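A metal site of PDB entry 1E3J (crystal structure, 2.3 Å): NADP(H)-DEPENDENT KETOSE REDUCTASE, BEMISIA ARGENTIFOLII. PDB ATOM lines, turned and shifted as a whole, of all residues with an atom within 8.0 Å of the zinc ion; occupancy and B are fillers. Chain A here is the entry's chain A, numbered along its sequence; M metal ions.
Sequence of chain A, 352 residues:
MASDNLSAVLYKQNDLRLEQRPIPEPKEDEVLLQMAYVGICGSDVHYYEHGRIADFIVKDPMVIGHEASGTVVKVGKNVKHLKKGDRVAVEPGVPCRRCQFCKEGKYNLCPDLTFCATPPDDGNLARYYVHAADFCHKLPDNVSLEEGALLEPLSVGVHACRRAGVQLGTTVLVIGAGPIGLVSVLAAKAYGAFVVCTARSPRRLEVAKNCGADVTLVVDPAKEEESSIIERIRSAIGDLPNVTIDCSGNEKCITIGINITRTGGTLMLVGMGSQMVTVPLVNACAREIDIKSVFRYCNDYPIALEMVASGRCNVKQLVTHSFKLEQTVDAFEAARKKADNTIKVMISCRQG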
ATOM      1  N   VAL A  94      34.166 -11.204 -18.407  1.00  0.00           N
ATOM      2  CA  VAL A  94      33.334 -10.749 -19.516  1.00  0.00           C
ATOM      3  C   VAL A  94      33.368 -11.854 -20.548  1.00  0.00           C
ATOM      4  O   VAL A  94      34.414 -12.167 -21.101  1.00  0.00           O
ATOM      5  CB  VAL A  94      33.856  -9.432 -20.105  1.00  0.00           C
ATOM      6  CG1 VAL A  94      32.959  -8.990 -21.250  1.00  0.00           C
ATOM      7  CG2 VAL A  94      33.875  -8.362 -18.999  1.00  0.00           C
ATOM      8  N   PRO A  95      32.213 -12.495 -20.801  1.00  0.00           N
ATOM      9  CA  PRO A  95      32.022 -13.586 -21.747  1.00  0.00           C
ATOM     10  C   PRO A  95      31.935 -13.164 -23.220  1.00  0.00           C
ATOM     11  O   PRO A  95      31.867 -11.981 -23.506  1.00  0.00           O
ATOM     12  CB  PRO A  95      30.740 -14.222 -21.246  1.00  0.00           C
ATOM     13  CG  PRO A  95      29.913 -13.024 -20.921  1.00  0.00           C
ATOM     14  CD  PRO A  95      30.941 -12.127 -20.168  1.00  0.00           C
ATOM     15  N   CYS A  96      31.903 -14.131 -24.150  1.00  0.00           N
ATOM     16  CA  CYS A  96      31.828 -13.800 -25.578  1.00  0.00           C
ATOM     17  C   CYS A  96      30.428 -13.370 -26.011  1.00  0.00           C
ATOM     18  O   CYS A  96      30.237 -12.678 -27.035  1.00  0.00           O
ATOM     19  CB  CYS A  96      32.303 -15.007 -26.440  1.00  0.00           C
ATOM     20  SG  CYS A  96      30.979 -16.268 -26.746  1.00  0.00           S
ATOM     21  N   ARG A  97      29.430 -13.770 -25.225  1.00  0.00           N
ATOM     22  CA  ARG A  97      28.033 -13.416 -25.482  1.00  0.00           C
ATOM     23  C   ARG A  97      27.445 -14.089 -26.738  1.00  0.00           C
ATOM     24  O   ARG A  97      26.378 -13.710 -27.174  1.00  0.00           O
ATOM     25  CB  ARG A  97      27.918 -11.899 -25.685  1.00  0.00           C
ATOM     26  CG  ARG A  97      28.473 -11.019 -24.603  1.00  0.00           C
ATOM     27  CD  ARG A  97      28.238  -9.583 -25.000  1.00  0.00           C
ATOM     28  NE  ARG A  97      28.248  -8.695 -23.849  1.00  0.00           N
ATOM     29  CZ  ARG A  97      29.325  -8.074 -23.406  1.00  0.00           C
ATOM     30  NH1 ARG A  97      30.481  -8.281 -24.041  1.00  0.00           N
ATOM     31  NH2 ARG A  97      29.244  -7.282 -22.338  1.00  0.00           N
ATOM     32  N   ARG A  98      28.126 -15.074 -27.310  1.00  0.00           N
ATOM     33  CA  ARG A  98      27.637 -15.699 -28.549  1.00  0.00           C
ATOM     34  C   ARG A  98      27.787 -17.211 -28.572  1.00  0.00           C
ATOM     35  O   ARG A  98      27.430 -17.840 -29.564  1.00  0.00           O
ATOM     36  CB  ARG A  98      28.404 -15.131 -29.756  1.00  0.00           C
ATOM     37  CG  ARG A  98      28.283 -13.602 -29.916  1.00  0.00           C
ATOM     38  CD  ARG A  98      29.266 -13.020 -30.975  1.00  0.00           C
ATOM     39  NE  ARG A  98      28.760 -11.736 -31.482  1.00  0.00           N
ATOM     40  CZ  ARG A  98      28.660 -10.623 -30.758  1.00  0.00           C
ATOM     41  NH1 ARG A  98      29.034 -10.593 -29.481  1.00  0.00           N
ATOM     42  NH2 ARG A  98      28.161  -9.521 -31.312  1.00  0.00           N
ATOM     43  N   CYS A  99      28.353 -17.817 -27.549  1.00  0.00           N
ATOM     44  CA  CYS A  99      28.431 -19.249 -27.629  1.00  0.00           C
ATOM     45  C   CYS A  99      27.143 -19.853 -26.975  1.00  0.00           C
ATOM     46  O   CYS A  99      26.266 -19.094 -26.499  1.00  0.00           O
ATOM     47  CB  CYS A  99      29.711 -19.753 -26.946  1.00  0.00           C
ATOM     48  SG  CYS A  99      29.650 -19.483 -25.204  1.00  0.00           S
ATOM     49  N   GLN A 100      27.022 -21.172 -26.972  1.00  0.00           N
ATOM     50  CA  GLN A 100      25.839 -21.793 -26.353  1.00  0.00           C
ATOM     51  C   GLN A 100      25.827 -21.562 -24.841  1.00  0.00           C
ATOM     52  O   GLN A 100      24.756 -21.470 -24.250  1.00  0.00           O
ATOM     53  CB  GLN A 100      25.788 -23.313 -26.608  1.00  0.00           C
ATOM     54  N   PHE A 101      27.007 -21.462 -24.195  1.00  0.00           N
ATOM     55  CA  PHE A 101      27.012 -21.230 -22.737  1.00  0.00           C
ATOM     56  C   PHE A 101      26.477 -19.856 -22.414  1.00  0.00           C
ATOM     57  O   PHE A 101      25.712 -19.715 -21.454  1.00  0.00           O
ATOM     58  CB  PHE A 101      28.413 -21.414 -22.142  1.00  0.00           C
ATOM     59  CG  PHE A 101      28.924 -22.826 -22.214  1.00  0.00           C
ATOM     60  CD1 PHE A 101      28.452 -23.790 -21.334  1.00  0.00           C
ATOM     61  CD2 PHE A 101      29.874 -23.191 -23.153  1.00  0.00           C
ATOM     62  CE1 PHE A 101      28.913 -25.111 -21.398  1.00  0.00           C
ATOM     63  CE2 PHE A 101      30.344 -24.499 -23.228  1.00  0.00           C
ATOM     64  CZ  PHE A 101      29.864 -25.453 -22.343  1.00  0.00           C
ATOM     65  N   CYS A 102      26.844 -18.844 -23.207  1.00  0.00           N
ATOM     66  CA  CYS A 102      26.328 -17.491 -22.945  1.00  0.00           C
ATOM     67  C   CYS A 102      24.830 -17.412 -23.307  1.00  0.00           C
ATOM     68  O   CYS A 102      24.043 -16.789 -22.615  1.00  0.00           O
ATOM     69  CB  CYS A 102      27.094 -16.418 -23.747  1.00  0.00           C
ATOM     70  SG  CYS A 102      28.966 -16.350 -23.475  1.00  0.00           S
ATOM     71  N   LYS A 103      24.421 -18.048 -24.404  1.00  0.00           N
ATOM     72  CA  LYS A 103      22.994 -17.962 -24.802  1.00  0.00           C
ATOM     73  C   LYS A 103      22.091 -18.685 -23.818  1.00  0.00           C
ATOM     74  O   LYS A 103      20.927 -18.323 -23.641  1.00  0.00           O
ATOM     75  CB  LYS A 103      22.795 -18.557 -26.196  1.00  0.00           C
ATOM     76  CG  LYS A 103      23.174 -17.616 -27.306  1.00  0.00           C
ATOM     77  CD  LYS A 103      23.262 -18.403 -28.623  1.00  0.00           C
ATOM     78  CE  LYS A 103      23.470 -17.484 -29.815  1.00  0.00           C
ATOM     79  NZ  LYS A 103      23.805 -18.391 -30.957  1.00  0.00           N
ATOM     80  N   LYS A 106      24.735 -19.373 -18.978  1.00  0.00           N
ATOM     81  CA  LYS A 106      25.867 -19.900 -18.185  1.00  0.00           C
ATOM     82  C   LYS A 106      27.111 -19.182 -18.658  1.00  0.00           C
ATOM     83  O   LYS A 106      28.076 -19.817 -19.074  1.00  0.00           O
ATOM     84  CB  LYS A 106      26.038 -21.402 -18.424  1.00  0.00           C
ATOM     85  CG  LYS A 106      24.804 -22.207 -17.973  1.00  0.00           C
ATOM     86  N   TYR A 107      27.118 -17.852 -18.606  1.00  0.00           N
ATOM     87  CA  TYR A 107      28.293 -17.184 -19.160  1.00  0.00           C
ATOM     88  C   TYR A 107      29.610 -17.414 -18.392  1.00  0.00           C
ATOM     89  O   TYR A 107      30.672 -17.344 -18.996  1.00  0.00           O
ATOM     90  CB  TYR A 107      28.018 -15.692 -19.405  1.00  0.00           C
ATOM     91  CG  TYR A 107      27.804 -14.877 -18.162  1.00  0.00           C
ATOM     92  CD1 TYR A 107      28.894 -14.559 -17.323  1.00  0.00           C
ATOM     93  CD2 TYR A 107      26.549 -14.422 -17.833  1.00  0.00           C
ATOM     94  CE1 TYR A 107      28.708 -13.766 -16.169  1.00  0.00           C
ATOM     95  CE2 TYR A 107      26.356 -13.648 -16.688  1.00  0.00           C
ATOM     96  CZ  TYR A 107      27.442 -13.325 -15.865  1.00  0.00           C
ATOM     97  OH  TYR A 107      27.226 -12.555 -14.727  1.00  0.00           O
ATOM     98  N   ASN A 108      29.540 -17.776 -17.106  1.00  0.00           N
ATOM     99  CA  ASN A 108      30.772 -18.062 -16.336  1.00  0.00           C
ATOM    100  C   ASN A 108      31.487 -19.270 -16.925  1.00  0.00           C
ATOM    101  O   ASN A 108      32.648 -19.496 -16.634  1.00  0.00           O
ATOM    102  CB  ASN A 108      30.483 -18.306 -14.855  1.00  0.00           C
ATOM    103  CG  ASN A 108      29.549 -19.479 -14.625  1.00  0.00           C
ATOM    104  OD1 ASN A 108      28.598 -19.705 -15.396  1.00  0.00           O
ATOM    105  ND2 ASN A 108      29.814 -20.227 -13.550  1.00  0.00           N
ATOM    106  N   LEU A 109      30.827 -20.039 -17.777  1.00  0.00           N
ATOM    107  CA  LEU A 109      31.478 -21.200 -18.384  1.00  0.00           C
ATOM    108  C   LEU A 109      31.875 -20.907 -19.838  1.00  0.00           C
ATOM    109  O   LEU A 109      32.345 -21.793 -20.546  1.00  0.00           O
ATOM    110  CB  LEU A 109      30.528 -22.395 -18.367  1.00  0.00           C
ATOM    111  CG  LEU A 109      30.000 -22.785 -16.978  1.00  0.00           C
ATOM    112  CD1 LEU A 109      29.112 -24.001 -17.090  1.00  0.00           C
ATOM    113  CD2 LEU A 109      31.211 -23.106 -16.075  1.00  0.00           C
ATOM    114  N   CYS A 110      31.666 -19.690 -20.292  1.00  0.00           N
ATOM    115  CA  CYS A 110      32.020 -19.355 -21.647  1.00  0.00           C
ATOM    116  C   CYS A 110      33.474 -19.756 -21.936  1.00  0.00           C
ATOM    117  O   CYS A 110      34.373 -19.456 -21.142  1.00  0.00           O
ATOM    118  CB  CYS A 110      31.874 -17.832 -21.851  1.00  0.00           C
ATOM    119  SG  CYS A 110      32.471 -17.306 -23.445  1.00  0.00           S
ATOM    120  N   PRO A 111      33.730 -20.429 -23.052  1.00  0.00           N
ATOM    121  CA  PRO A 111      35.139 -20.789 -23.280  1.00  0.00           C
ATOM    122  C   PRO A 111      36.065 -19.615 -23.638  1.00  0.00           C
ATOM    123  O   PRO A 111      37.281 -19.734 -23.475  1.00  0.00           O
ATOM    124  CB  PRO A 111      35.086 -21.842 -24.397  1.00  0.00           C
ATOM    125  CG  PRO A 111      33.833 -21.493 -25.112  1.00  0.00           C
ATOM    126  CD  PRO A 111      32.868 -21.160 -23.979  1.00  0.00           C
ATOM    127  N   ASP A 112      35.490 -18.520 -24.141  1.00  0.00           N
ATOM    128  CA  ASP A 112      36.306 -17.366 -24.512  1.00  0.00           C
ATOM    129  C   ASP A 112      36.114 -16.272 -23.469  1.00  0.00           C
ATOM    130  O   ASP A 112      36.172 -15.078 -23.775  1.00  0.00           O
ATOM    131  CB  ASP A 112      35.931 -16.818 -25.892  1.00  0.00           C
ATOM    132  CG  ASP A 112      36.085 -17.862 -26.997  1.00  0.00           C
ATOM    133  OD1 ASP A 112      37.014 -18.706 -26.934  1.00  0.00           O
ATOM    134  OD2 ASP A 112      35.281 -17.820 -27.945  1.00  0.00           O
ATOM    135  N   LEU A 113      35.849 -16.689 -22.237  1.00  0.00           N
ATOM    136  CA  LEU A 113      35.683 -15.718 -21.174  1.00  0.00           C
ATOM    137  C   LEU A 113      37.017 -14.963 -20.953  1.00  0.00           C
ATOM    138  O   LEU A 113      38.102 -15.559 -21.012  1.00  0.00           O
ATOM    139  CB  LEU A 113      35.324 -16.443 -19.854  1.00  0.00           C
ATOM    140  CG  LEU A 113      35.016 -15.628 -18.602  1.00  0.00           C
ATOM    141  CD1 LEU A 113      33.570 -15.141 -18.589  1.00  0.00           C
ATOM    142  CD2 LEU A 113      35.208 -16.533 -17.420  1.00  0.00           C
HETATM  143 ZN    ZN M   1      30.370 -17.381 -24.706  1.00  0.00          ZN
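SG of Cys 110 sits close to N of Asp 112. N of Leu 113 sits close to SG of Cys 110. SG of Cys 102 lies close to N of Arg 97 (3.2 Å). The backbone carbonyl oxygen (O) of Cys 96 is in hydrogen-bond range of the guanidinium group (NH1) of Arg 98 (3.4 Å). SG of Cys 99 lies close to N of Phe 101 (3.5 Å).
Arg 97 touches the zinc ion. Five residues have an atom within 4 Å of the zinc ion: Cys 96, Arg 97, Cys 99, Cys 102 and Cys 110. The nearest printed residue that does not touch the zinc ion is Arg 98 (4.1 Å).
The zinc ion is bound by SG of Cys 102 (2.1 Å), SG of Cys 99 (2.3 Å), SG of Cys 96 (2.4 Å) and SG of Cys 110 (2.5 Å). The zinc ion has four donor atoms within binding distance.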
